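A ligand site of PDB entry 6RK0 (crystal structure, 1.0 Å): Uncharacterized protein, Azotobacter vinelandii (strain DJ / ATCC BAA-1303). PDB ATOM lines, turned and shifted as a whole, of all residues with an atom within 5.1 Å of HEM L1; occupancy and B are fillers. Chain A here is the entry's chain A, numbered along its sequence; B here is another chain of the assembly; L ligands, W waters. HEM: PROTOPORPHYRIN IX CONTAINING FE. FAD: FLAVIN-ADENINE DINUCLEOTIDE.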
ATOM      1  N   ARG A  23       7.457  -1.988  26.834  1.00  0.00           N
ATOM      2  CA  ARG A  23       8.518  -1.788  25.862  1.00  0.00           C
ATOM      3  C   ARG A  23       8.137  -0.709  24.862  1.00  0.00           C
ATOM      4  O   ARG A  23       6.991  -0.631  24.396  1.00  0.00           O
ATOM      5  CB  ARG A  23       8.826  -3.106  25.144  1.00  0.00           C
ATOM      6  CG  ARG A  23       9.167  -4.221  26.147  1.00  0.00           C
ATOM      7  CD  ARG A  23      10.268  -5.177  25.689  1.00  0.00           C
ATOM      8  NE  ARG A  23      11.580  -4.509  25.618  1.00  0.00           N
ATOM      9  CZ  ARG A  23      12.468  -4.422  26.619  1.00  0.00           C
ATOM     10  NH1 ARG A  23      13.568  -3.739  26.386  1.00  0.00           N
ATOM     11  NH2 ARG A  23      12.235  -4.937  27.831  1.00  0.00           N
ATOM     12  N   TYR A  24       9.092   0.153  24.522  1.00  0.00           N
ATOM     13  CA  TYR A  24       8.815   1.224  23.569  1.00  0.00           C
ATOM     14  C   TYR A  24       7.550   1.996  23.978  1.00  0.00           C
ATOM     15  O   TYR A  24       6.705   2.372  23.162  1.00  0.00           O
ATOM     16  CB  TYR A  24       8.773   0.725  22.123  1.00  0.00           C
ATOM     17  CG  TYR A  24      10.139   0.645  21.466  1.00  0.00           C
ATOM     18  CD1 TYR A  24      11.228  -0.028  22.061  1.00  0.00           C
ATOM     19  CD2 TYR A  24      10.357   1.278  20.271  1.00  0.00           C
ATOM     20  CE1 TYR A  24      12.467  -0.030  21.484  1.00  0.00           C
ATOM     21  CE2 TYR A  24      11.602   1.276  19.673  1.00  0.00           C
ATOM     22  CZ  TYR A  24      12.640   0.628  20.286  1.00  0.00           C
ATOM     23  OH  TYR A  24      13.901   0.622  19.719  1.00  0.00           O
ATOM     24  N   LEU A  27       5.654   4.912  22.303  1.00  0.00           N
ATOM     25  CA  LEU A  27       4.762   4.693  21.168  1.00  0.00           C
ATOM     26  C   LEU A  27       3.328   4.404  21.582  1.00  0.00           C
ATOM     27  O   LEU A  27       2.452   4.257  20.720  1.00  0.00           O
ATOM     28  CB  LEU A  27       5.265   3.561  20.294  1.00  0.00           C
ATOM     29  CG  LEU A  27       6.653   3.803  19.714  1.00  0.00           C
ATOM     30  CD1 LEU A  27       7.002   2.557  18.845  1.00  0.00           C
ATOM     31  CD2 LEU A  27       6.793   5.086  18.951  1.00  0.00           C
ATOM     32  N   LEU A  98       8.391  -0.262   5.965  1.00  0.00           N
ATOM     33  CA  LEU A  98       9.642  -0.843   6.437  1.00  0.00           C
ATOM     34  C   LEU A  98      10.617   0.303   6.704  1.00  0.00           C
ATOM     35  O   LEU A  98      10.840   1.152   5.833  1.00  0.00           O
ATOM     36  CB  LEU A  98      10.211  -1.801   5.403  1.00  0.00           C
ATOM     37  CG  LEU A  98      11.505  -2.497   5.828  1.00  0.00           C
ATOM     38  CD1 LEU A  98      11.299  -3.404   7.025  1.00  0.00           C
ATOM     39  CD2 LEU A  98      12.105  -3.281   4.676  1.00  0.00           C
ATOM     40  N   ALA A 104      21.509  -2.385  11.863  1.00  0.00           N
ATOM     41  CA  ALA A 104      20.490  -3.431  11.834  1.00  0.00           C
ATOM     42  C   ALA A 104      19.585  -3.363  13.066  1.00  0.00           C
ATOM     43  O   ALA A 104      18.363  -3.534  12.967  1.00  0.00           O
ATOM     44  CB  ALA A 104      21.174  -4.777  11.733  1.00  0.00           C
ATOM     45  N   TYR A 105      20.184  -3.094  14.234  1.00  0.00           N
ATOM     46  CA  TYR A 105      19.461  -3.063  15.486  1.00  0.00           C
ATOM     47  C   TYR A 105      18.333  -2.051  15.452  1.00  0.00           C
ATOM     48  O   TYR A 105      17.339  -2.244  16.169  1.00  0.00           O
ATOM     49  CB  TYR A 105      20.478  -2.670  16.575  1.00  0.00           C
ATOM     50  CG  TYR A 105      19.991  -2.680  17.989  1.00  0.00           C
ATOM     51  CD1 TYR A 105      19.851  -3.877  18.692  1.00  0.00           C
ATOM     52  CD2 TYR A 105      19.749  -1.501  18.662  1.00  0.00           C
ATOM     53  CE1 TYR A 105      19.505  -3.917  20.016  1.00  0.00           C
ATOM     54  CE2 TYR A 105      19.365  -1.520  20.004  1.00  0.00           C
ATOM     55  CZ  TYR A 105      19.255  -2.739  20.677  1.00  0.00           C
ATOM     56  OH  TYR A 105      18.897  -2.795  22.027  1.00  0.00           O
ATOM     57  N   PHE A 107      16.621  -1.101  12.613  1.00  0.00           N
ATOM     58  CA  PHE A 107      15.565  -1.330  11.636  1.00  0.00           C
ATOM     59  C   PHE A 107      14.229  -1.437  12.378  1.00  0.00           C
ATOM     60  O   PHE A 107      14.160  -1.777  13.569  1.00  0.00           O
ATOM     61  CB  PHE A 107      15.807  -2.629  10.834  1.00  0.00           C
ATOM     62  CG  PHE A 107      16.628  -2.435   9.590  1.00  0.00           C
ATOM     63  CD1 PHE A 107      17.865  -1.815   9.624  1.00  0.00           C
ATOM     64  CD2 PHE A 107      16.147  -2.864   8.350  1.00  0.00           C
ATOM     65  CE1 PHE A 107      18.631  -1.649   8.462  1.00  0.00           C
ATOM     66  CE2 PHE A 107      16.903  -2.702   7.185  1.00  0.00           C
ATOM     67  CZ  PHE A 107      18.137  -2.082   7.274  1.00  0.00           C
ATOM     68  N   ASN A 108      13.138  -1.157  11.665  1.00  0.00           N
ATOM     69  CA  ASN A 108      11.878  -1.130  12.361  1.00  0.00           C
ATOM     70  C   ASN A 108      10.763  -1.179  11.339  1.00  0.00           C
ATOM     71  O   ASN A 108      11.009  -1.444  10.147  1.00  0.00           O
ATOM     72  CB  ASN A 108      11.804   0.084  13.313  1.00  0.00           C
ATOM     73  CG  ASN A 108      11.093  -0.241  14.585  1.00  0.00           C
ATOM     74  OD1 ASN A 108       9.876  -0.420  14.603  1.00  0.00           O
ATOM     75  ND2 ASN A 108      11.840  -0.361  15.659  1.00  0.00           N
ATOM     76  N   CYS A 109       9.542  -0.950  11.798  1.00  0.00           N
ATOM     77  CA  CYS A 109       8.381  -0.846  10.937  1.00  0.00           C
ATOM     78  C   CYS A 109       7.563   0.361  11.384  1.00  0.00           C
ATOM     79  O   CYS A 109       7.569   0.698  12.571  1.00  0.00           O
ATOM     80  CB  CYS A 109       7.479  -2.075  11.078  1.00  0.00           C
ATOM     81  SG  CYS A 109       8.165  -3.769  10.934  1.00  0.00           S
ATOM     82  N   PHE A 111       3.658   1.397  11.747  1.00  0.00           N
ATOM     83  CA  PHE A 111       2.507   0.522  11.990  1.00  0.00           C
ATOM     84  C   PHE A 111       1.509   1.244  12.878  1.00  0.00           C
ATOM     85  O   PHE A 111       1.839   2.232  13.565  1.00  0.00           O
ATOM     86  CB  PHE A 111       2.938  -0.793  12.672  1.00  0.00           C
ATOM     87  CG  PHE A 111       3.526  -0.620  14.038  1.00  0.00           C
ATOM     88  CD1 PHE A 111       2.722  -0.619  15.183  1.00  0.00           C
ATOM     89  CD2 PHE A 111       4.896  -0.440  14.207  1.00  0.00           C
ATOM     90  CE1 PHE A 111       3.291  -0.442  16.451  1.00  0.00           C
ATOM     91  CE2 PHE A 111       5.454  -0.280  15.499  1.00  0.00           C
ATOM     92  CZ  PHE A 111       4.626  -0.299  16.600  1.00  0.00           C
ATOM     93  N   LYS A 172      -0.270   0.890  20.010  1.00  0.00           N
ATOM     94  CA  LYS A 172       1.054   1.376  19.707  1.00  0.00           C
ATOM     95  C   LYS A 172       1.029   1.845  18.270  1.00  0.00           C
ATOM     96  O   LYS A 172       0.430   1.199  17.407  1.00  0.00           O
ATOM     97  CB  LYS A 172       2.184   0.311  19.904  1.00  0.00           C
ATOM     98  CG  LYS A 172       2.432  -0.040  21.366  1.00  0.00           C
ATOM     99  CD  LYS A 172       3.397  -1.177  21.541  1.00  0.00           C
ATOM    100  CE  LYS A 172       4.882  -0.867  21.239  1.00  0.00           C
ATOM    101  NZ  LYS A 172       5.724  -2.094  21.432  1.00  0.00           N
ATOM    102  N   PHE B  61       7.254  -9.528  12.975  1.00  0.00           N
ATOM    103  CA  PHE B  61       7.856 -10.027  11.751  1.00  0.00           C
ATOM    104  C   PHE B  61       8.356 -11.456  11.961  1.00  0.00           C
ATOM    105  O   PHE B  61       8.655 -11.864  13.085  1.00  0.00           O
ATOM    106  CB  PHE B  61       8.999  -9.134  11.296  1.00  0.00           C
ATOM    107  CG  PHE B  61       8.541  -8.063  10.298  1.00  0.00           C
ATOM    108  CD1 PHE B  61       9.347  -7.626   9.279  1.00  0.00           C
ATOM    109  CD2 PHE B  61       7.209  -7.535  10.332  1.00  0.00           C
ATOM    110  CE1 PHE B  61       8.927  -6.644   8.376  1.00  0.00           C
ATOM    111  CE2 PHE B  61       6.763  -6.561   9.413  1.00  0.00           C
ATOM    112  CZ  PHE B  61       7.655  -6.096   8.446  1.00  0.00           C
ATOM    113  N   HIS B  72      12.090 -12.249  16.308  1.00  0.00           N
ATOM    114  CA  HIS B  72      13.063 -11.620  17.201  1.00  0.00           C
ATOM    115  C   HIS B  72      12.378 -10.569  18.049  1.00  0.00           C
ATOM    116  O   HIS B  72      11.272 -10.106  17.743  1.00  0.00           O
ATOM    117  CB  HIS B  72      14.196 -10.930  16.383  1.00  0.00           C
ATOM    118  CG  HIS B  72      13.865  -9.532  15.942  1.00  0.00           C
ATOM    119  ND1 HIS B  72      12.868  -9.222  15.042  1.00  0.00           N
ATOM    120  CD2 HIS B  72      14.408  -8.343  16.305  1.00  0.00           C
ATOM    121  CE1 HIS B  72      12.792  -7.900  14.915  1.00  0.00           C
ATOM    122  NE2 HIS B  72      13.718  -7.350  15.661  1.00  0.00           N
ATOM    123  N   GLY B  73      13.065 -10.183  19.111  1.00  0.00           N
ATOM    124  CA  GLY B  73      12.639  -9.051  19.913  1.00  0.00           C
ATOM    125  C   GLY B  73      13.620  -8.882  21.055  1.00  0.00           C
ATOM    126  O   GLY B  73      14.788  -9.279  20.945  1.00  0.00           O
ATOM    127  N   SER B  74      13.189  -8.282  22.150  1.00  0.00           N
ATOM    128  CA  SER B  74      14.087  -8.039  23.263  1.00  0.00           C
ATOM    129  C   SER B  74      14.444  -9.337  23.980  1.00  0.00           C
ATOM    130  O   SER B  74      13.563 -10.143  24.284  1.00  0.00           O
ATOM    131  CB  SER B  74      13.422  -7.097  24.261  1.00  0.00           C
ATOM    132  OG  SER B  74      14.203  -6.983  25.440  1.00  0.00           O
ATOM    133  N   LEU B 133      19.912 -13.463  12.293  1.00  0.00           N
ATOM    134  CA  LEU B 133      19.494 -12.063  12.120  1.00  0.00           C
ATOM    135  C   LEU B 133      19.969 -11.505  10.780  1.00  0.00           C
ATOM    136  O   LEU B 133      19.239 -10.737  10.122  1.00  0.00           O
ATOM    137  CB  LEU B 133      20.019 -11.210  13.276  1.00  0.00           C
ATOM    138  CG  LEU B 133      19.307 -11.481  14.625  1.00  0.00           C
ATOM    139  CD1 LEU B 133      20.105 -10.894  15.772  1.00  0.00           C
ATOM    140  CD2 LEU B 133      17.878 -10.948  14.633  1.00  0.00           C
ATOM    141  N   PHE B 136      17.535 -12.734   8.280  1.00  0.00           N
ATOM    142  CA  PHE B 136      16.309 -11.941   8.351  1.00  0.00           C
ATOM    143  C   PHE B 136      16.435 -10.667   7.528  1.00  0.00           C
ATOM    144  O   PHE B 136      15.635 -10.390   6.628  1.00  0.00           O
ATOM    145  CB  PHE B 136      16.073 -11.625   9.829  1.00  0.00           C
ATOM    146  CG  PHE B 136      14.897 -10.694  10.149  1.00  0.00           C
ATOM    147  CD1 PHE B 136      13.718 -10.713   9.387  1.00  0.00           C
ATOM    148  CD2 PHE B 136      14.983  -9.856  11.233  1.00  0.00           C
ATOM    149  CE1 PHE B 136      12.642  -9.897   9.742  1.00  0.00           C
ATOM    150  CE2 PHE B 136      13.910  -9.057  11.603  1.00  0.00           C
ATOM    151  CZ  PHE B 136      12.772  -9.087  10.838  1.00  0.00           C
ATOM    152  N   VAL B 137      17.472  -9.876   7.797  1.00  0.00           N
ATOM    153  CA  VAL B 137      17.638  -8.593   7.102  1.00  0.00           C
ATOM    154  C   VAL B 137      17.803  -8.823   5.613  1.00  0.00           C
ATOM    155  O   VAL B 137      17.165  -8.134   4.795  1.00  0.00           O
ATOM    156  CB  VAL B 137      18.812  -7.813   7.715  1.00  0.00           C
ATOM    157  CG1 VAL B 137      19.195  -6.613   6.868  1.00  0.00           C
ATOM    158  CG2 VAL B 137      18.491  -7.403   9.140  1.00  0.00           C
ATOM    159  N   LEU B 140      14.804  -9.585   3.517  1.00  0.00           N
ATOM    160  CA  LEU B 140      13.972  -8.438   3.170  1.00  0.00           C
ATOM    161  C   LEU B 140      14.619  -7.630   2.061  1.00  0.00           C
ATOM    162  O   LEU B 140      13.950  -7.252   1.095  1.00  0.00           O
ATOM    163  CB  LEU B 140      13.744  -7.565   4.388  1.00  0.00           C
ATOM    164  CG  LEU B 140      12.952  -8.196   5.520  1.00  0.00           C
ATOM    165  CD1 LEU B 140      12.913  -7.279   6.717  1.00  0.00           C
ATOM    166  CD2 LEU B 140      11.545  -8.509   5.050  1.00  0.00           C
ATOM    167  N   TRP B 145      22.619  -6.344   5.159  1.00  0.00           N
ATOM    168  CA  TRP B 145      23.315  -6.433   6.451  1.00  0.00           C
ATOM    169  C   TRP B 145      24.747  -5.942   6.322  1.00  0.00           C
ATOM    170  O   TRP B 145      25.238  -5.242   7.200  1.00  0.00           O
ATOM    171  CB  TRP B 145      23.315  -7.895   6.883  1.00  0.00           C
ATOM    172  CG  TRP B 145      24.058  -8.234   8.135  1.00  0.00           C
ATOM    173  CD1 TRP B 145      25.353  -8.622   8.247  1.00  0.00           C
ATOM    174  CD2 TRP B 145      23.506  -8.335   9.440  1.00  0.00           C
ATOM    175  NE1 TRP B 145      25.636  -8.922   9.536  1.00  0.00           N
ATOM    176  CE2 TRP B 145      24.514  -8.772  10.307  1.00  0.00           C
ATOM    177  CE3 TRP B 145      22.228  -8.084   9.948  1.00  0.00           C
ATOM    178  CZ2 TRP B 145      24.293  -8.967  11.683  1.00  0.00           C
ATOM    179  CZ3 TRP B 145      22.006  -8.300  11.281  1.00  0.00           C
ATOM    180  CH2 TRP B 145      23.019  -8.717  12.136  1.00  0.00           C
ATOM    181  N   VAL B 151      27.553  -4.397  13.330  1.00  0.00           N
ATOM    182  CA  VAL B 151      26.780  -4.714  14.524  1.00  0.00           C
ATOM    183  C   VAL B 151      27.677  -4.784  15.752  1.00  0.00           C
ATOM    184  O   VAL B 151      28.814  -5.271  15.699  1.00  0.00           O
ATOM    185  CB  VAL B 151      25.948  -6.003  14.304  1.00  0.00           C
ATOM    186  CG1 VAL B 151      26.824  -7.260  14.223  1.00  0.00           C
ATOM    187  CG2 VAL B 151      24.895  -6.176  15.409  1.00  0.00           C
ATOM    188  N   GLU B 155      24.388  -5.305  20.938  1.00  0.00           N
ATOM    189  CA  GLU B 155      23.124  -5.339  20.185  1.00  0.00           C
ATOM    190  C   GLU B 155      22.667  -6.788  19.988  1.00  0.00           C
ATOM    191  O   GLU B 155      21.497  -7.096  20.216  1.00  0.00           O
ATOM    192  CB  GLU B 155      23.295  -4.613  18.842  1.00  0.00           C
ATOM    193  CG  GLU B 155      23.430  -3.125  19.032  1.00  0.00           C
ATOM    194  CD  GLU B 155      23.883  -2.346  17.809  1.00  0.00           C
ATOM    195  OE1 GLU B 155      24.572  -2.920  16.930  1.00  0.00           O
ATOM    196  OE2 GLU B 155      23.537  -1.145  17.751  1.00  0.00           O
ATOM    197  N   ILE B 156      23.589  -7.685  19.587  1.00  0.00           N
ATOM    198  CA  ILE B 156      23.245  -9.094  19.449  1.00  0.00           C
ATOM    199  C   ILE B 156      22.766  -9.639  20.783  1.00  0.00           C
ATOM    200  O   ILE B 156      21.758 -10.357  20.865  1.00  0.00           O
ATOM    201  CB  ILE B 156      24.452  -9.879  18.898  1.00  0.00           C
ATOM    202  CG1 ILE B 156      24.864  -9.420  17.499  1.00  0.00           C
ATOM    203  CG2 ILE B 156      24.166 -11.397  18.936  1.00  0.00           C
ATOM    204  CD1 ILE B 156      23.847  -9.621  16.418  1.00  0.00           C
ATOM    205  N   ALA B 158      21.428  -8.219  23.297  1.00  0.00           N
ATOM    206  CA  ALA B 158      20.170  -7.651  23.737  1.00  0.00           C
ATOM    207  C   ALA B 158      18.972  -8.217  22.975  1.00  0.00           C
ATOM    208  O   ALA B 158      17.838  -7.846  23.295  1.00  0.00           O
ATOM    209  CB  ALA B 158      20.214  -6.122  23.567  1.00  0.00           C
ATOM    210  N   THR B 159      19.183  -9.071  21.993  1.00  0.00           N
ATOM    211  CA  THR B 159      18.129  -9.553  21.104  1.00  0.00           C
ATOM    212  C   THR B 159      17.828 -11.010  21.429  1.00  0.00           C
ATOM    213  O   THR B 159      18.751 -11.821  21.579  1.00  0.00           O
ATOM    214  CB  THR B 159      18.588  -9.412  19.656  1.00  0.00           C
ATOM    215  OG1 THR B 159      19.004  -8.060  19.425  1.00  0.00           O
ATOM    216  CG2 THR B 159      17.478  -9.723  18.684  1.00  0.00           C
HETATM  217  CHA HEM L   1      12.348  -4.756  18.423  1.00  0.00           C
HETATM  218  CHB HEM L   1      11.523  -4.603  13.704  1.00  0.00           C
HETATM  219  CHC HEM L   1      15.974  -6.183  12.891  1.00  0.00           C
HETATM  220  CHD HEM L   1      16.915  -6.031  17.588  1.00  0.00           C
HETATM  221  C1A HEM L   1      11.746  -4.568  17.203  1.00  0.00           C
HETATM  222  C2A HEM L   1      10.387  -4.087  17.041  1.00  0.00           C
HETATM  223  C3A HEM L   1      10.146  -4.036  15.732  1.00  0.00           C
HETATM  224  C4A HEM L   1      11.363  -4.500  15.061  1.00  0.00           C
HETATM  225  CMA HEM L   1       8.908  -3.593  14.949  1.00  0.00           C
HETATM  226  CAA HEM L   1       9.447  -3.657  18.166  1.00  0.00           C
HETATM  227  CBA HEM L   1       9.729  -2.237  18.677  1.00  0.00           C
HETATM  228  CGA HEM L   1       8.513  -1.788  19.451  1.00  0.00           C
HETATM  229  O1A HEM L   1       7.758  -0.895  18.966  1.00  0.00           O
HETATM  230  O2A HEM L   1       8.253  -2.324  20.554  1.00  0.00           O
HETATM  231  C1B HEM L   1      12.675  -5.017  13.060  1.00  0.00           C
HETATM  232  C2B HEM L   1      12.819  -5.157  11.620  1.00  0.00           C
HETATM  233  C3B HEM L   1      14.039  -5.605  11.405  1.00  0.00           C
HETATM  234  C4B HEM L   1      14.703  -5.723  12.693  1.00  0.00           C
HETATM  235  CMB HEM L   1      11.733  -4.893  10.584  1.00  0.00           C
HETATM  236  CAB HEM L   1      14.785  -5.958  10.112  1.00  0.00           C
HETATM  237  CBB HEM L   1      14.386  -5.686   8.879  1.00  0.00           C
HETATM  238  C1C HEM L   1      16.631  -6.310  14.098  1.00  0.00           C
HETATM  239  C2C HEM L   1      17.984  -6.746  14.291  1.00  0.00           C
HETATM  240  C3C HEM L   1      18.273  -6.663  15.574  1.00  0.00           C
HETATM  241  C4C HEM L   1      17.075  -6.158  16.232  1.00  0.00           C
HETATM  242  CMC HEM L   1      18.851  -7.295  13.174  1.00  0.00           C
HETATM  243  CAC HEM L   1      19.560  -6.959  16.304  1.00  0.00           C
HETATM  244  CBC HEM L   1      20.732  -6.696  15.729  1.00  0.00           C
HETATM  245  C1D HEM L   1      15.734  -5.735  18.244  1.00  0.00           C
HETATM  246  C2D HEM L   1      15.564  -5.631  19.677  1.00  0.00           C
HETATM  247  C3D HEM L   1      14.294  -5.273  19.893  1.00  0.00           C
HETATM  248  C4D HEM L   1      13.657  -5.135  18.594  1.00  0.00           C
HETATM  249  CMD HEM L   1      16.649  -5.925  20.722  1.00  0.00           C
HETATM  250  CAD HEM L   1      13.642  -4.961  21.240  1.00  0.00           C
HETATM  251  CBD HEM L   1      13.719  -3.436  21.497  1.00  0.00           C
HETATM  252  CGD HEM L   1      13.370  -3.144  22.934  1.00  0.00           C
HETATM  253  O1D HEM L   1      12.145  -3.144  23.259  1.00  0.00           O
HETATM  254  O2D HEM L   1      14.257  -2.855  23.760  1.00  0.00           O
HETATM  255  NA  HEM L   1      12.340  -4.806  15.983  1.00  0.00           N
HETATM  256  NB  HEM L   1      13.848  -5.351  13.689  1.00  0.00           N
HETATM  257  NC  HEM L   1      16.070  -5.966  15.312  1.00  0.00           N
HETATM  258  ND  HEM L   1      14.557  -5.409  17.600  1.00  0.00           N
HETATM  259 FE   HEM L   1      14.186  -5.413  15.657  1.00  0.00          FE
HETATM  260  PA  FAD L   2       4.860  -5.358  26.744  1.00  0.00           P
HETATM  261  O1A FAD L   2       5.136  -3.902  26.723  1.00  0.00           O
HETATM  262  O2A FAD L   2       5.517  -6.180  27.801  1.00  0.00           O
HETATM  263  O5B FAD L   2       3.289  -5.601  26.753  1.00  0.00           O
HETATM  264  C5B FAD L   2       2.493  -5.029  27.820  1.00  0.00           C
HETATM  265  C4B FAD L   2       1.172  -4.588  27.259  1.00  0.00           C
HETATM  266  O4B FAD L   2       1.393  -3.610  26.215  1.00  0.00           O
HETATM  267  C3B FAD L   2       0.353  -5.668  26.562  1.00  0.00           C
HETATM  268  O3B FAD L   2      -0.303  -6.515  27.478  1.00  0.00           O
HETATM  269  C2B FAD L   2      -0.558  -4.836  25.667  1.00  0.00           C
HETATM  270  O2B FAD L   2      -1.663  -4.384  26.407  1.00  0.00           O
HETATM  271  C1B FAD L   2       0.355  -3.688  25.252  1.00  0.00           C
HETATM  272  N9A FAD L   2       0.978  -3.886  23.942  1.00  0.00           N
HETATM  273  C8A FAD L   2       2.135  -4.546  23.651  1.00  0.00           C
HETATM  274  N7A FAD L   2       2.384  -4.616  22.369  1.00  0.00           N
HETATM  275  C5A FAD L   2       1.308  -3.972  21.774  1.00  0.00           C
HETATM  276  C6A FAD L   2       0.980  -3.713  20.430  1.00  0.00           C
HETATM  277  N6A FAD L   2       1.719  -4.113  19.368  1.00  0.00           N
HETATM  278  N1A FAD L   2      -0.179  -3.049  20.186  1.00  0.00           N
HETATM  279  C2A FAD L   2      -0.934  -2.669  21.216  1.00  0.00           C
HETATM  280  N3A FAD L   2      -0.733  -2.854  22.528  1.00  0.00           N
HETATM  281  C4A FAD L   2       0.433  -3.514  22.741  1.00  0.00           C
HETATM  282  N1  FAD L   2       8.050  -6.604  17.999  1.00  0.00           N
HETATM  283  C2  FAD L   2       9.220  -7.299  17.967  1.00  0.00           C
HETATM  284  O2  FAD L   2       9.867  -7.546  19.001  1.00  0.00           O
HETATM  285  N3  FAD L   2       9.704  -7.777  16.765  1.00  0.00           N
HETATM  286  C4  FAD L   2       9.097  -7.610  15.558  1.00  0.00           C
HETATM  287  O4  FAD L   2       9.555  -8.111  14.530  1.00  0.00           O
HETATM  288  C4X FAD L   2       7.890  -6.821  15.606  1.00  0.00           C
HETATM  289  N5  FAD L   2       7.238  -6.567  14.455  1.00  0.00           N
HETATM  290  C5X FAD L   2       6.030  -5.884  14.523  1.00  0.00           C
HETATM  291  C6  FAD L   2       5.290  -5.671  13.348  1.00  0.00           C
HETATM  292  C7  FAD L   2       4.062  -5.017  13.369  1.00  0.00           C
HETATM  293  C7M FAD L   2       3.299  -4.784  12.080  1.00  0.00           C
HETATM  294  C8  FAD L   2       3.544  -4.583  14.603  1.00  0.00           C
HETATM  295  C8M FAD L   2       2.194  -3.956  14.702  1.00  0.00           C
HETATM  296  C9  FAD L   2       4.293  -4.764  15.772  1.00  0.00           C
HETATM  297  C9A FAD L   2       5.504  -5.426  15.746  1.00  0.00           C
HETATM  298  N10 FAD L   2       6.280  -5.615  16.913  1.00  0.00           N
HETATM  299  C10 FAD L   2       7.428  -6.383  16.880  1.00  0.00           C
HETATM  300  C1' FAD L   2       5.832  -5.140  18.236  1.00  0.00           C
HETATM  301  C2' FAD L   2       5.125  -6.224  19.034  1.00  0.00           C
HETATM  302  O2' FAD L   2       3.780  -6.321  18.597  1.00  0.00           O
HETATM  303  C3' FAD L   2       5.167  -5.901  20.524  1.00  0.00           C
HETATM  304  O3' FAD L   2       4.564  -4.627  20.742  1.00  0.00           O
HETATM  305  C4' FAD L   2       6.573  -5.901  21.108  1.00  0.00           C
HETATM  306  O4' FAD L   2       7.237  -7.116  20.735  1.00  0.00           O
HETATM  307  C5' FAD L   2       6.537  -5.835  22.612  1.00  0.00           C
HETATM  308  O5' FAD L   2       5.703  -6.892  23.127  1.00  0.00           O
HETATM  309  P   FAD L   2       5.708  -7.275  24.656  1.00  0.00           P
HETATM  310  O1P FAD L   2       7.106  -7.549  25.152  1.00  0.00           O
HETATM  311  O2P FAD L   2       4.655  -8.355  24.850  1.00  0.00           O
HETATM  312  O3P FAD L   2       5.174  -5.907  25.291  1.00  0.00           O
HETATM  313  O   HOH W   1      14.823  -3.427  15.620  1.00  0.00           O
HETATM  314  O   HOH W   2       9.998  -4.059  21.827  1.00  0.00           O
HETATM  315  O   HOH W   3      13.721  -1.767  17.742  1.00  0.00           O
HETATM  316  O   HOH W   4      16.825  -3.514  23.748  1.00  0.00           O
HETATM  317  O   HOH W   5      16.209  -2.507  18.772  1.00  0.00           O
HETATM  318  O   HOH W   6       5.021  -2.268  18.547  1.00  0.00           O
HETATM  319  O   HOH W   7      14.027  -0.176  25.090  1.00  0.00           O
HETATM  320  O   HOH W   8       8.766   0.622  16.925  1.00  0.00           O
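The guanidinium group (NH1) of Arg 23 lies close to the side-chain hydroxyl (OG) of Ser 74 of chain B, at 3.4 Å.
OG1 of Thr 159 of chain B lies within hydrogen-bond range of O of Glu 155 of chain B (2.8 Å).
An oxygen (O4) of FAD L2 is in hydrogen-bond range of the backbone NH (N) of Phe 61 of chain B (3.1 Å).
N of Arg 23 is in hydrogen-bond range of O1A of FAD L2 (3.0 Å).
An iron atom (FE) of HEM L1 is bound by a ring nitrogen (NE2) of His 72 of chain B (2.0 Å).
The side-chain amino group (NZ) of Lys 172 is in salt-bridge range of an oxygen (O2A) of HEM L1.
The side-chain amino group of Lys 172 lies within hydrogen-bond range of an oxygen (O3') of FAD L2.
The backbone carbonyl oxygen of His 72 of chain B sits at hydrogen-bond distance from a nitrogen (N3) of FAD L2.
NE of Arg 23 is in salt-bridge range of O1D of HEM L1 (2.8 Å).
CD1 of Tyr 24 touches O1D of HEM L1, at 3.5 Å.
Leu 27 touches HEM L1.
Leu 98 touches HEM L1 (CD1 to CMB, 3.9 Å).
O of Ala 104 touches C1C of HEM L1, 3.5 Å away.
CE1 of Tyr 105 touches CMD of HEM L1 (3.6 Å).
CD2 of Phe 107 touches CBB of HEM L1, 3.4 Å away.
Asn 108 touches HEM L1 (OD1 to CMA, 3.3 Å).
SG of Cys 109 touches CMB of HEM L1, 3.8 Å away.
Phe 111 touches HEM L1 (CZ to O1A, 3.97 Å).
Phe 61 of chain B touches HEM L1.
Gly 73 of chain B touches HEM L1.
Ser 74 of chain B touches HEM L1 (N to CAD, 3.5 Å).
Phe 136 of chain B touches HEM L1.
Leu 140 of chain B touches HEM L1.
CZ3 of Trp 145 of chain B touches CMC of HEM L1 (3.8 Å).
O of Ala 158 of chain B touches CMD of HEM L1 (3.4 Å).
Thr 159 of chain B touches HEM L1 (OG1 to CAC, 3.4 Å).
20 residues have an atom within 4 Å of HEM L1: Arg 23, Tyr 24, Leu 27, Leu 98, Ala 104, Tyr 105, Phe 107, Asn 108, Cys 109, Phe 111, Lys 172, Phe 61 of chain B, His 72 of chain B, Gly 73 of chain B, Ser 74 of chain B, Phe 136 of chain B, Leu 140 of chain B, Trp 145 of chain B, Ala 158 of chain B and Thr 159 of chain B.
Water W4 bridges an oxygen (O2D) of HEM L1 (2.7 Å) and the side-chain hydroxyl (OH) of Tyr 105 (2.8 Å).
Water W8 bridges O1A of HEM L1 (2.7 Å) and OD1 of Asn 108 (2.8 Å).
Water W6 lies within hydrogen-bond range of NZ of Lys 172 (3.0 Å), O1A of HEM L1 (3.1 Å) and O3' of FAD L2 (3.3 Å).
Water W3 lies within hydrogen-bond range of OH of Tyr 24 (3.1 Å) and ND2 of Asn 108 (3.1 Å).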
